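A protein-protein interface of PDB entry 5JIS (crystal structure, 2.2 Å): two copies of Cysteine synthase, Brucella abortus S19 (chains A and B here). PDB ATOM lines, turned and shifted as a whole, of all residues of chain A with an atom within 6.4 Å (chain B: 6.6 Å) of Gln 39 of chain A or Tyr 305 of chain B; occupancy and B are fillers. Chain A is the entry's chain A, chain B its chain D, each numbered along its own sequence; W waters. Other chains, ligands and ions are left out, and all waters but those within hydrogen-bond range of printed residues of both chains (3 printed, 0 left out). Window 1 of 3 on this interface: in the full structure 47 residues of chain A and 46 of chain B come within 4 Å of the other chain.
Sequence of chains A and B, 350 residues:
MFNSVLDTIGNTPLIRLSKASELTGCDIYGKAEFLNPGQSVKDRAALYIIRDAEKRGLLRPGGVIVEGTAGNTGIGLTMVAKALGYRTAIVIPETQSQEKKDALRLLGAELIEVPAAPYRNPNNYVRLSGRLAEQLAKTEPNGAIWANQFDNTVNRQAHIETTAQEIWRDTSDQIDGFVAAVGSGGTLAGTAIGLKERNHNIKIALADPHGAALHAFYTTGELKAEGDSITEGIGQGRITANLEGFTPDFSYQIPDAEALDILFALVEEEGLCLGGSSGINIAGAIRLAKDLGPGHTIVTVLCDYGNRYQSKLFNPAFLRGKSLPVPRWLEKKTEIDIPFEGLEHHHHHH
Tyr 305 of chain B touches three residues of chain A. Of the printed residues of chain B, Asn 36 of chain A touches Tyr 305. Printed residues of chain B within 4 Å of Asn 307 of chain A: Gln 39 (3.1 Å). The nearest printed residue of chain B that does not touch Leu 35 of chain A is Asn 36 of chain B (4.02 Å).
Leu 35 of chain A touches Leu 35 of chain B (O to CD2, 3.6 Å). Asn 36 of chain A touches Tyr 305 of chain B. Pro 37 of chain A touches Leu 35 of chain B. CG of Gln 39 of chain A touches OH of Tyr 305 of chain B, at 3.4 Å. O of Asn 36 of chain B touches OH of Tyr 305 of chain A (3.7 Å). Tyr 305 of chain A touches Gln 39 of chain B (CE2 to NE2, 3.1 Å).
Water W1 lies within hydrogen-bond range of OH of Tyr 305 of chain B (2.7 Å), O of Asn 36 of chain A (2.9 Å) and O of Phe 34 of chain A (2.9 Å). Water W3 lies within hydrogen-bond range of OH of Tyr 305 of chain A, O of Phe 34 of chain B, O of Asn 36 of chain B and NE2 of Gln 39 of chain B. Water W2 lies within hydrogen-bond range of the side-chain amide oxygen (OE1) of Gln 39 of chain A (2.9 Å) and the side-chain amide oxygen (OD1) of Asn 307 of chain B (3.4 Å).
The backbone carbonyl oxygen (O) of Pro 37 of chain A is in hydrogen-bond range of the side-chain hydroxyl (OH) of Tyr 305 of chain B. OE1 of Gln 39 of chain A is in hydrogen-bond range of NE2 of Gln 39 of chain B. The side-chain amide oxygen of Asn 307 of chain B lies within hydrogen-bond range of the side-chain amide nitrogen of Gln 39 of chain A, at 3.4 Å. OE1 of Gln 39 of chain B sits at hydrogen-bond distance from ND2 of Asn 307 of chain A (3.1 Å).
Hydrophobic or aromatic side chains of chain A that line the printed part of chain B: Leu 35 and Tyr 305. Of the 19 printed residues of chain B, 5 touch a printed residue of chain A. Hydrophobic or aromatic side chains of chain B within 4 Å of the printed part of chain A: Leu 35 and Tyr 305.
The side-chain carboxylate (OE1) of Glu 33 of chain A is in hydrogen-bond range of the side-chain amide nitrogen (ND2) of Asn 36 of chain A (2.9 Å). ND2 of Asn 36 of chain A sits at hydrogen-bond distance from O of Ser 40 of chain A (3.1 Å). The side-chain amide nitrogen (ND2) of Asn 36 of chain B sits at hydrogen-bond distance from the backbone carbonyl oxygen (O) of Ser 40 of chain B (3.1 Å). The side-chain amide oxygen (OE1) of Gln 39 of chain B lies within hydrogen-bond range of the guanidinium group (NH2) of Arg 308 of chain B, at 3.1 Å.
Leu 35 of chain A touches its own counterpart, Leu 35 of chain B. Asn 36 of chain A touches Tyr 305 of chain B, and with the chains exchanged Tyr 305 of chain A touches Asn 36 of chain B. Gln 39 of chain A touches its own counterpart, Gln 39 of chain B. Gln 39 of chain A touches Asn 307 of chain B, and with the chains exchanged Asn 307 of chain A touches Gln 39 of chain B. Positions printed for both chains: 34, 35, 36, 39, 40, 303, 304, 305, 307 and 308.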
ATOM      1  N   GLU A  33       1.153  21.098 -29.174  1.00  0.00           N
ATOM      2  CA  GLU A  33       1.126  19.639 -29.003  1.00  0.00           C
ATOM      3  C   GLU A  33       1.871  19.139 -27.766  1.00  0.00           C
ATOM      4  O   GLU A  33       1.670  17.999 -27.326  1.00  0.00           O
ATOM      5  CB  GLU A  33       1.695  18.943 -30.250  1.00  0.00           C
ATOM      6  CG  GLU A  33       0.836  19.117 -31.480  1.00  0.00           C
ATOM      7  CD  GLU A  33      -0.544  18.517 -31.287  1.00  0.00           C
ATOM      8  OE1 GLU A  33      -0.635  17.299 -30.998  1.00  0.00           O
ATOM      9  OE2 GLU A  33      -1.538  19.256 -31.416  1.00  0.00           O
ATOM     10  N   PHE A  34       2.738  19.994 -27.233  1.00  0.00           N
ATOM     11  CA  PHE A  34       3.356  19.779 -25.933  1.00  0.00           C
ATOM     12  C   PHE A  34       2.351  19.710 -24.784  1.00  0.00           C
ATOM     13  O   PHE A  34       2.682  19.138 -23.740  1.00  0.00           O
ATOM     14  CB  PHE A  34       4.467  20.812 -25.645  1.00  0.00           C
ATOM     15  CG  PHE A  34       4.019  22.256 -25.657  1.00  0.00           C
ATOM     16  CD1 PHE A  34       3.520  22.861 -24.494  1.00  0.00           C
ATOM     17  CD2 PHE A  34       4.160  23.037 -26.804  1.00  0.00           C
ATOM     18  CE1 PHE A  34       3.137  24.204 -24.481  1.00  0.00           C
ATOM     19  CE2 PHE A  34       3.778  24.378 -26.797  1.00  0.00           C
ATOM     20  CZ  PHE A  34       3.262  24.955 -25.637  1.00  0.00           C
ATOM     21  N   LEU A  35       1.137  20.250 -24.972  1.00  0.00           N
ATOM     22  CA  LEU A  35       0.086  20.151 -23.964  1.00  0.00           C
ATOM     23  C   LEU A  35      -0.725  18.834 -23.983  1.00  0.00           C
ATOM     24  O   LEU A  35      -1.696  18.697 -23.236  1.00  0.00           O
ATOM     25  CB  LEU A  35      -0.848  21.363 -24.029  1.00  0.00           C
ATOM     26  CG  LEU A  35      -0.171  22.711 -23.734  1.00  0.00           C
ATOM     27  CD1 LEU A  35      -1.222  23.800 -23.791  1.00  0.00           C
ATOM     28  CD2 LEU A  35       0.522  22.717 -22.365  1.00  0.00           C
ATOM     29  N   ASN A  36      -0.324  17.876 -24.812  1.00  0.00           N
ATOM     30  CA  ASN A  36      -0.846  16.514 -24.727  1.00  0.00           C
ATOM     31  C   ASN A  36      -0.326  15.847 -23.453  1.00  0.00           C
ATOM     32  O   ASN A  36       0.747  16.221 -22.975  1.00  0.00           O
ATOM     33  CB  ASN A  36      -0.391  15.715 -25.959  1.00  0.00           C
ATOM     34  CG  ASN A  36      -1.165  16.075 -27.209  1.00  0.00           C
ATOM     35  OD1 ASN A  36      -2.381  16.085 -27.194  1.00  0.00           O
ATOM     36  ND2 ASN A  36      -0.465  16.350 -28.303  1.00  0.00           N
ATOM     37  N   PRO A  37      -1.057  14.857 -22.899  1.00  0.00           N
ATOM     38  CA  PRO A  37      -0.634  14.215 -21.621  1.00  0.00           C
ATOM     39  C   PRO A  37       0.677  13.424 -21.655  1.00  0.00           C
ATOM     40  O   PRO A  37       1.296  13.227 -20.602  1.00  0.00           O
ATOM     41  CB  PRO A  37      -1.810  13.274 -21.287  1.00  0.00           C
ATOM     42  CG  PRO A  37      -2.439  13.007 -22.605  1.00  0.00           C
ATOM     43  CD  PRO A  37      -2.320  14.278 -23.392  1.00  0.00           C
ATOM     44  N   GLY A  38       1.082  12.968 -22.843  1.00  0.00           N
ATOM     45  CA  GLY A  38       2.405  12.383 -23.061  1.00  0.00           C
ATOM     46  C   GLY A  38       3.460  13.421 -23.418  1.00  0.00           C
ATOM     47  O   GLY A  38       4.597  13.063 -23.711  1.00  0.00           O
ATOM     48  N   GLN A  39       3.069  14.702 -23.390  1.00  0.00           N
ATOM     49  CA  GLN A  39       3.945  15.864 -23.603  1.00  0.00           C
ATOM     50  C   GLN A  39       4.497  15.996 -25.027  1.00  0.00           C
ATOM     51  O   GLN A  39       5.495  16.672 -25.250  1.00  0.00           O
ATOM     52  CB  GLN A  39       5.061  15.937 -22.536  1.00  0.00           C
ATOM     53  CG  GLN A  39       4.549  15.848 -21.099  1.00  0.00           C
ATOM     54  CD  GLN A  39       5.647  15.892 -20.046  1.00  0.00           C
ATOM     55  OE1 GLN A  39       6.509  16.761 -20.073  1.00  0.00           O
ATOM     56  NE2 GLN A  39       5.607  14.960 -19.098  1.00  0.00           N
ATOM     57  N   SER A  40       3.833  15.372 -25.999  1.00  0.00           N
ATOM     58  CA  SER A  40       4.225  15.552 -27.396  1.00  0.00           C
ATOM     59  C   SER A  40       3.106  15.249 -28.369  1.00  0.00           C
ATOM     60  O   SER A  40       2.093  14.667 -28.005  1.00  0.00           O
ATOM     61  CB  SER A  40       5.444  14.688 -27.755  1.00  0.00           C
ATOM     62  OG  SER A  40       5.053  13.413 -28.247  1.00  0.00           O
ATOM     63  N   VAL A  41       3.349  15.652 -29.615  1.00  0.00           N
ATOM     64  CA  VAL A  41       2.522  15.333 -30.790  1.00  0.00           C
ATOM     65  C   VAL A  41       2.222  13.836 -30.981  1.00  0.00           C
ATOM     66  O   VAL A  41       1.169  13.480 -31.527  1.00  0.00           O
ATOM     67  CB  VAL A  41       3.189  15.883 -32.081  1.00  0.00           C
ATOM     68  CG1 VAL A  41       4.506  15.171 -32.395  1.00  0.00           C
ATOM     69  CG2 VAL A  41       2.232  15.797 -33.268  1.00  0.00           C
ATOM     70  N   ASP A  43       1.172  11.526 -29.080  1.00  0.00           N
ATOM     71  CA  ASP A  43      -0.038  10.969 -28.456  1.00  0.00           C
ATOM     72  C   ASP A  43      -1.146  10.629 -29.443  1.00  0.00           C
ATOM     73  O   ASP A  43      -1.872   9.668 -29.238  1.00  0.00           O
ATOM     74  CB  ASP A  43      -0.599  11.919 -27.401  1.00  0.00           C
ATOM     75  CG  ASP A  43       0.278  12.009 -26.170  1.00  0.00           C
ATOM     76  OD1 ASP A  43       1.355  11.370 -26.096  1.00  0.00           O
ATOM     77  OD2 ASP A  43      -0.128  12.727 -25.247  1.00  0.00           O
ATOM     78  N   ASN A  72       9.597   9.789 -28.502  1.00  0.00           N
ATOM     79  CA  ASN A  72       8.243  10.283 -28.256  1.00  0.00           C
ATOM     80  C   ASN A  72       7.153   9.271 -28.608  1.00  0.00           C
ATOM     81  O   ASN A  72       6.168   9.157 -27.875  1.00  0.00           O
ATOM     82  CB  ASN A  72       7.964  11.624 -28.954  1.00  0.00           C
ATOM     83  CG  ASN A  72       8.525  12.836 -28.189  1.00  0.00           C
ATOM     84  OD1 ASN A  72       8.559  12.859 -26.961  1.00  0.00           O
ATOM     85  ND2 ASN A  72       8.930  13.847 -28.916  1.00  0.00           N
ATOM     86  N   ILE A  75       6.920   6.973 -25.805  1.00  0.00           N
ATOM     87  CA  ILE A  75       6.286   7.655 -24.676  1.00  0.00           C
ATOM     88  C   ILE A  75       4.761   7.661 -24.824  1.00  0.00           C
ATOM     89  O   ILE A  75       4.058   7.260 -23.901  1.00  0.00           O
ATOM     90  CB  ILE A  75       6.844   9.073 -24.465  1.00  0.00           C
ATOM     91  CG1 ILE A  75       8.311   8.979 -24.005  1.00  0.00           C
ATOM     92  CG2 ILE A  75       6.048   9.822 -23.403  1.00  0.00           C
ATOM     93  CD1 ILE A  75       9.066  10.281 -24.103  1.00  0.00           C
ATOM     94  N   MET A  79       2.116   5.397 -22.485  1.00  0.00           N
ATOM     95  CA  MET A  79       1.011   6.017 -21.740  1.00  0.00           C
ATOM     96  C   MET A  79      -0.354   5.388 -22.089  1.00  0.00           C
ATOM     97  O   MET A  79      -1.131   5.013 -21.197  1.00  0.00           O
ATOM     98  CB  MET A  79       0.966   7.520 -21.994  1.00  0.00           C
ATOM     99  CG  MET A  79      -0.250   8.220 -21.391  1.00  0.00           C
ATOM    100  SD  MET A  79      -0.380   9.930 -21.916  1.00  0.00           S
ATOM    101  CE  MET A  79      -0.893   9.703 -23.617  1.00  0.00           C
ATOM    102  N   CYS A 303       5.932  20.850 -31.211  1.00  0.00           N
ATOM    103  CA  CYS A 303       5.788  19.391 -31.085  1.00  0.00           C
ATOM    104  C   CYS A 303       5.992  18.845 -29.679  1.00  0.00           C
ATOM    105  O   CYS A 303       5.353  17.855 -29.317  1.00  0.00           O
ATOM    106  CB  CYS A 303       6.720  18.651 -32.049  1.00  0.00           C
ATOM    107  SG  CYS A 303       6.663  19.247 -33.752  1.00  0.00           S
ATOM    108  N   ASP A 304       6.885  19.478 -28.911  1.00  0.00           N
ATOM    109  CA  ASP A 304       7.233  19.038 -27.559  1.00  0.00           C
ATOM    110  C   ASP A 304       8.088  20.099 -26.822  1.00  0.00           C
ATOM    111  O   ASP A 304       8.452  21.123 -27.403  1.00  0.00           O
ATOM    112  CB  ASP A 304       7.902  17.647 -27.575  1.00  0.00           C
ATOM    113  CG  ASP A 304       9.279  17.624 -28.229  1.00  0.00           C
ATOM    114  OD1 ASP A 304       9.759  18.656 -28.752  1.00  0.00           O
ATOM    115  OD2 ASP A 304       9.897  16.537 -28.197  1.00  0.00           O
ATOM    116  N   TYR A 305       8.380  19.842 -25.550  1.00  0.00           N
ATOM    117  CA  TYR A 305       9.109  20.785 -24.700  1.00  0.00           C
ATOM    118  C   TYR A 305      10.623  20.743 -24.899  1.00  0.00           C
ATOM    119  O   TYR A 305      11.214  19.698 -25.213  1.00  0.00           O
ATOM    120  CB  TYR A 305       8.833  20.509 -23.218  1.00  0.00           C
ATOM    121  CG  TYR A 305       7.516  20.994 -22.695  1.00  0.00           C
ATOM    122  CD1 TYR A 305       7.348  22.329 -22.288  1.00  0.00           C
ATOM    123  CD2 TYR A 305       6.447  20.118 -22.534  1.00  0.00           C
ATOM    124  CE1 TYR A 305       6.135  22.782 -21.772  1.00  0.00           C
ATOM    125  CE2 TYR A 305       5.233  20.554 -22.018  1.00  0.00           C
ATOM    126  CZ  TYR A 305       5.079  21.884 -21.634  1.00  0.00           C
ATOM    127  OH  TYR A 305       3.871  22.302 -21.122  1.00  0.00           O
ATOM    128  N   ASN A 307      12.745  20.916 -22.467  1.00  0.00           N
ATOM    129  CA  ASN A 307      13.301  20.083 -21.382  1.00  0.00           C
ATOM    130  C   ASN A 307      13.551  18.623 -21.774  1.00  0.00           C
ATOM    131  O   ASN A 307      14.343  17.935 -21.139  1.00  0.00           O
ATOM    132  CB  ASN A 307      12.454  20.163 -20.082  1.00  0.00           C
ATOM    133  CG  ASN A 307      11.041  19.611 -20.239  1.00  0.00           C
ATOM    134  OD1 ASN A 307      10.853  18.480 -20.682  1.00  0.00           O
ATOM    135  ND2 ASN A 307      10.035  20.399 -19.837  1.00  0.00           N
ATOM    136  N   ARG A 308      12.881  18.167 -22.822  1.00  0.00           N
ATOM    137  CA  ARG A 308      13.083  16.829 -23.365  1.00  0.00           C
ATOM    138  C   ARG A 308      14.422  16.644 -24.100  1.00  0.00           C
ATOM    139  O   ARG A 308      14.782  15.517 -24.439  1.00  0.00           O
ATOM    140  CB  ARG A 308      11.890  16.483 -24.268  1.00  0.00           C
ATOM    141  CG  ARG A 308      11.790  15.035 -24.711  1.00  0.00           C
ATOM    142  CD  ARG A 308      10.343  14.576 -24.845  1.00  0.00           C
ATOM    143  NE  ARG A 308       9.753  14.348 -23.527  1.00  0.00           N
ATOM    144  CZ  ARG A 308       8.536  13.860 -23.292  1.00  0.00           C
ATOM    145  NH1 ARG A 308       7.704  13.530 -24.290  1.00  0.00           N
ATOM    146  NH2 ARG A 308       8.137  13.725 -22.035  1.00  0.00           N
ATOM    147  N   PHE B  34      -1.109  19.422 -14.352  1.00  0.00           N
ATOM    148  CA  PHE B  34       0.066  19.118 -15.161  1.00  0.00           C
ATOM    149  C   PHE B  34      -0.038  19.509 -16.642  1.00  0.00           C
ATOM    150  O   PHE B  34       0.989  19.670 -17.313  1.00  0.00           O
ATOM    151  CB  PHE B  34       0.491  17.650 -15.006  1.00  0.00           C
ATOM    152  CG  PHE B  34      -0.545  16.638 -15.412  1.00  0.00           C
ATOM    153  CD1 PHE B  34      -0.638  16.209 -16.730  1.00  0.00           C
ATOM    154  CD2 PHE B  34      -1.367  16.042 -14.459  1.00  0.00           C
ATOM    155  CE1 PHE B  34      -1.545  15.223 -17.100  1.00  0.00           C
ATOM    156  CE2 PHE B  34      -2.292  15.066 -14.823  1.00  0.00           C
ATOM    157  CZ  PHE B  34      -2.378  14.650 -16.151  1.00  0.00           C
ATOM    158  N   LEU B  35      -1.263  19.672 -17.133  1.00  0.00           N
ATOM    159  CA  LEU B  35      -1.521  20.139 -18.487  1.00  0.00           C
ATOM    160  C   LEU B  35      -1.533  21.665 -18.646  1.00  0.00           C
ATOM    161  O   LEU B  35      -1.922  22.160 -19.693  1.00  0.00           O
ATOM    162  CB  LEU B  35      -2.854  19.557 -18.990  1.00  0.00           C
ATOM    163  CG  LEU B  35      -2.914  18.033 -19.052  1.00  0.00           C
ATOM    164  CD1 LEU B  35      -4.246  17.617 -19.643  1.00  0.00           C
ATOM    165  CD2 LEU B  35      -1.775  17.466 -19.887  1.00  0.00           C
ATOM    166  N   ASN B  36      -1.166  22.409 -17.606  1.00  0.00           N
ATOM    167  CA  ASN B  36      -0.772  23.810 -17.774  1.00  0.00           C
ATOM    168  C   ASN B  36       0.571  23.922 -18.529  1.00  0.00           C
ATOM    169  O   ASN B  36       1.414  23.015 -18.447  1.00  0.00           O
ATOM    170  CB  ASN B  36      -0.664  24.490 -16.411  1.00  0.00           C
ATOM    171  CG  ASN B  36      -2.016  24.754 -15.774  1.00  0.00           C
ATOM    172  OD1 ASN B  36      -2.948  25.213 -16.432  1.00  0.00           O
ATOM    173  ND2 ASN B  36      -2.124  24.478 -14.483  1.00  0.00           N
ATOM    174  N   GLN B  39       3.470  23.350 -16.628  1.00  0.00           N
ATOM    175  CA  GLN B  39       3.468  21.946 -16.202  1.00  0.00           C
ATOM    176  C   GLN B  39       3.149  21.741 -14.726  1.00  0.00           C
ATOM    177  O   GLN B  39       3.398  20.664 -14.183  1.00  0.00           O
ATOM    178  CB  GLN B  39       4.775  21.238 -16.557  1.00  0.00           C
ATOM    179  CG  GLN B  39       5.308  21.547 -17.957  1.00  0.00           C
ATOM    180  CD  GLN B  39       6.116  20.398 -18.522  1.00  0.00           C
ATOM    181  OE1 GLN B  39       7.326  20.386 -18.423  1.00  0.00           O
ATOM    182  NE2 GLN B  39       5.436  19.413 -19.091  1.00  0.00           N
ATOM    183  N   SER B  40       2.580  22.750 -14.082  1.00  0.00           N
ATOM    184  CA  SER B  40       2.107  22.594 -12.724  1.00  0.00           C
ATOM    185  C   SER B  40       0.963  23.521 -12.403  1.00  0.00           C
ATOM    186  O   SER B  40       0.670  24.460 -13.139  1.00  0.00           O
ATOM    187  CB  SER B  40       3.229  22.803 -11.699  1.00  0.00           C
ATOM    188  OG  SER B  40       3.375  24.166 -11.323  1.00  0.00           O
ATOM    189  N   CYS B 273       1.685   9.541 -14.617  1.00  0.00           N
ATOM    190  CA  CYS B 273       2.947   9.579 -13.894  1.00  0.00           C
ATOM    191  C   CYS B 273       3.099  10.968 -13.308  1.00  0.00           C
ATOM    192  O   CYS B 273       3.477  11.904 -14.024  1.00  0.00           O
ATOM    193  CB  CYS B 273       4.131   9.259 -14.799  1.00  0.00           C
ATOM    194  SG  CYS B 273       5.685   9.366 -13.870  1.00  0.00           S
ATOM    195  N   LEU B 274       2.831  11.074 -12.005  1.00  0.00           N
ATOM    196  CA  LEU B 274       2.599  12.346 -11.321  1.00  0.00           C
ATOM    197  C   LEU B 274       3.543  12.527 -10.147  1.00  0.00           C
ATOM    198  O   LEU B 274       4.185  11.556  -9.697  1.00  0.00           O
ATOM    199  CB  LEU B 274       1.163  12.378 -10.803  1.00  0.00           C
ATOM    200  CG  LEU B 274       0.062  12.024 -11.801  1.00  0.00           C
ATOM    201  CD1 LEU B 274      -1.277  12.035 -11.097  1.00  0.00           C
ATOM    202  CD2 LEU B 274       0.052  12.980 -12.983  1.00  0.00           C
ATOM    203  N   GLY B 275       3.600  13.760  -9.635  1.00  0.00           N
ATOM    204  CA  GLY B 275       4.474  14.101  -8.509  1.00  0.00           C
ATOM    205  C   GLY B 275       3.912  13.618  -7.180  1.00  0.00           C
ATOM    206  O   GLY B 275       2.772  13.137  -7.102  1.00  0.00           O
ATOM    207  N   GLY B 276       4.702  13.775  -6.119  1.00  0.00           N
ATOM    208  CA  GLY B 276       4.351  13.217  -4.821  1.00  0.00           C
ATOM    209  C   GLY B 276       3.092  13.795  -4.219  1.00  0.00           C
ATOM    210  O   GLY B 276       2.316  13.063  -3.591  1.00  0.00           O
ATOM    211  N   SER B 278       0.451  14.624  -5.676  1.00  0.00           N
ATOM    212  CA  SER B 278      -0.684  13.917  -6.279  1.00  0.00           C
ATOM    213  C   SER B 278      -0.986  12.603  -5.551  1.00  0.00           C
ATOM    214  O   SER B 278      -2.150  12.249  -5.371  1.00  0.00           O
ATOM    215  CB  SER B 278      -0.449  13.643  -7.772  1.00  0.00           C
ATOM    216  OG  SER B 278      -0.264  14.839  -8.519  1.00  0.00           O
ATOM    217  N   LEU B 302      -4.230  16.967  -9.491  1.00  0.00           N
ATOM    218  CA  LEU B 302      -3.034  16.298  -9.999  1.00  0.00           C
ATOM    219  C   LEU B 302      -2.056  17.406 -10.387  1.00  0.00           C
ATOM    220  O   LEU B 302      -2.117  17.950 -11.498  1.00  0.00           O
ATOM    221  CB  LEU B 302      -3.394  15.417 -11.188  1.00  0.00           C
ATOM    222  CG  LEU B 302      -4.608  14.505 -10.972  1.00  0.00           C
ATOM    223  CD1 LEU B 302      -4.916  13.749 -12.254  1.00  0.00           C
ATOM    224  CD2 LEU B 302      -4.411  13.558  -9.789  1.00  0.00           C
ATOM    225  N   CYS B 303      -1.167  17.732  -9.445  1.00  0.00           N
ATOM    226  CA  CYS B 303      -0.509  19.037  -9.392  1.00  0.00           C
ATOM    227  C   CYS B 303       0.615  19.218 -10.406  1.00  0.00           C
ATOM    228  O   CYS B 303       0.826  20.330 -10.892  1.00  0.00           O
ATOM    229  CB  CYS B 303       0.046  19.301  -7.997  1.00  0.00           C
ATOM    230  SG  CYS B 303      -1.152  19.122  -6.656  1.00  0.00           S
ATOM    231  N   ASP B 304       1.350  18.143 -10.684  1.00  0.00           N
ATOM    232  CA  ASP B 304       2.428  18.180 -11.667  1.00  0.00           C
ATOM    233  C   ASP B 304       2.834  16.767 -12.081  1.00  0.00           C
ATOM    234  O   ASP B 304       2.293  15.795 -11.555  1.00  0.00           O
ATOM    235  CB  ASP B 304       3.623  19.018 -11.150  1.00  0.00           C
ATOM    236  CG  ASP B 304       4.340  18.411  -9.936  1.00  0.00           C
ATOM    237  OD1 ASP B 304       3.940  17.350  -9.438  1.00  0.00           O
ATOM    238  OD2 ASP B 304       5.339  19.033  -9.474  1.00  0.00           O
ATOM    239  N   TYR B 305       3.761  16.668 -13.032  1.00  0.00           N
ATOM    240  CA  TYR B 305       4.288  15.388 -13.511  1.00  0.00           C
ATOM    241  C   TYR B 305       5.359  14.808 -12.588  1.00  0.00           C
ATOM    242  O   TYR B 305       6.058  15.529 -11.886  1.00  0.00           O
ATOM    243  CB  TYR B 305       4.932  15.535 -14.884  1.00  0.00           C
ATOM    244  CG  TYR B 305       3.993  15.650 -16.074  1.00  0.00           C
ATOM    245  CD1 TYR B 305       3.270  14.539 -16.543  1.00  0.00           C
ATOM    246  CD2 TYR B 305       3.879  16.854 -16.776  1.00  0.00           C
ATOM    247  CE1 TYR B 305       2.438  14.647 -17.661  1.00  0.00           C
ATOM    248  CE2 TYR B 305       3.049  16.971 -17.886  1.00  0.00           C
ATOM    249  CZ  TYR B 305       2.342  15.871 -18.337  1.00  0.00           C
ATOM    250  OH  TYR B 305       1.542  16.022 -19.446  1.00  0.00           O
ATOM    251  N   GLY B 306       5.519  13.493 -12.666  1.00  0.00           N
ATOM    252  CA  GLY B 306       6.505  12.766 -11.890  1.00  0.00           C
ATOM    253  C   GLY B 306       7.919  12.854 -12.427  1.00  0.00           C
ATOM    254  O   GLY B 306       8.863  12.528 -11.700  1.00  0.00           O
ATOM    255  N   ASN B 307       8.066  13.295 -13.676  1.00  0.00           N
ATOM    256  CA  ASN B 307       9.377  13.461 -14.331  1.00  0.00           C
ATOM    257  C   ASN B 307      10.361  14.357 -13.566  1.00  0.00           C
ATOM    258  O   ASN B 307      11.559  14.079 -13.516  1.00  0.00           O
ATOM    259  CB  ASN B 307       9.195  14.034 -15.746  1.00  0.00           C
ATOM    260  CG  ASN B 307       8.348  13.143 -16.628  1.00  0.00           C
ATOM    261  OD1 ASN B 307       7.124  13.238 -16.619  1.00  0.00           O
ATOM    262  ND2 ASN B 307       8.995  12.263 -17.386  1.00  0.00           N
ATOM    263  N   ARG B 308       9.838  15.411 -12.954  1.00  0.00           N
ATOM    264  CA  ARG B 308      10.640  16.314 -12.126  1.00  0.00           C
ATOM    265  C   ARG B 308      11.187  15.698 -10.815  1.00  0.00           C
ATOM    266  O   ARG B 308      12.082  16.277 -10.204  1.00  0.00           O
ATOM    267  CB  ARG B 308       9.839  17.597 -11.821  1.00  0.00           C
ATOM    268  CG  ARG B 308       9.965  18.637 -12.924  1.00  0.00           C
ATOM    269  CD  ARG B 308       8.878  19.713 -12.888  1.00  0.00           C
ATOM    270  NE  ARG B 308       8.763  20.332 -14.210  1.00  0.00           N
ATOM    271  CZ  ARG B 308       8.012  21.389 -14.529  1.00  0.00           C
ATOM    272  NH1 ARG B 308       7.257  22.037 -13.620  1.00  0.00           N
ATOM    273  NH2 ARG B 308       8.032  21.805 -15.793  1.00  0.00           N
ATOM    274  N   TYR B 309      10.665  14.543 -10.395  1.00  0.00           N
ATOM    275  CA  TYR B 309      11.049  13.915  -9.122  1.00  0.00           C
ATOM    276  C   TYR B 309      11.753  12.587  -9.348  1.00  0.00           C
ATOM    277  O   TYR B 309      11.952  11.807  -8.424  1.00  0.00           O
ATOM    278  CB  TYR B 309       9.799  13.680  -8.282  1.00  0.00           C
ATOM    279  CG  TYR B 309       8.978  14.926  -8.080  1.00  0.00           C
ATOM    280  CD1 TYR B 309       9.294  15.826  -7.073  1.00  0.00           C
ATOM    281  CD2 TYR B 309       7.901  15.218  -8.907  1.00  0.00           C
ATOM    282  CE1 TYR B 309       8.546  16.980  -6.883  1.00  0.00           C
ATOM    283  CE2 TYR B 309       7.153  16.365  -8.723  1.00  0.00           C
ATOM    284  CZ  TYR B 309       7.481  17.244  -7.704  1.00  0.00           C
ATOM    285  OH  TYR B 309       6.754  18.390  -7.497  1.00  0.00           O
ATOM    286  N   PHE B 314      11.059   8.394  -7.882  1.00  0.00           N
ATOM    287  CA  PHE B 314      11.070   7.200  -8.748  1.00  0.00           C
ATOM    288  C   PHE B 314      12.490   6.627  -8.900  1.00  0.00           C
ATOM    289  O   PHE B 314      12.851   6.071  -9.952  1.00  0.00           O
ATOM    290  CB  PHE B 314      10.473   7.537 -10.121  1.00  0.00           C
ATOM    291  CG  PHE B 314       9.026   7.964 -10.068  1.00  0.00           C
ATOM    292  CD1 PHE B 314       8.010   7.028 -10.190  1.00  0.00           C
ATOM    293  CD2 PHE B 314       8.685   9.305  -9.903  1.00  0.00           C
ATOM    294  CE1 PHE B 314       6.682   7.415 -10.143  1.00  0.00           C
ATOM    295  CE2 PHE B 314       7.352   9.698  -9.856  1.00  0.00           C
ATOM    296  CZ  PHE B 314       6.353   8.751  -9.972  1.00  0.00           C
HETATM  297  O   HOH W   1       1.924  18.103 -21.100  1.00  0.00           O
HETATM  298  O   HOH W   2       8.010  16.394 -17.657  1.00  0.00           O
HETATM  299  O   HOH W   3       2.313  20.457 -19.735  1.00  0.00           O
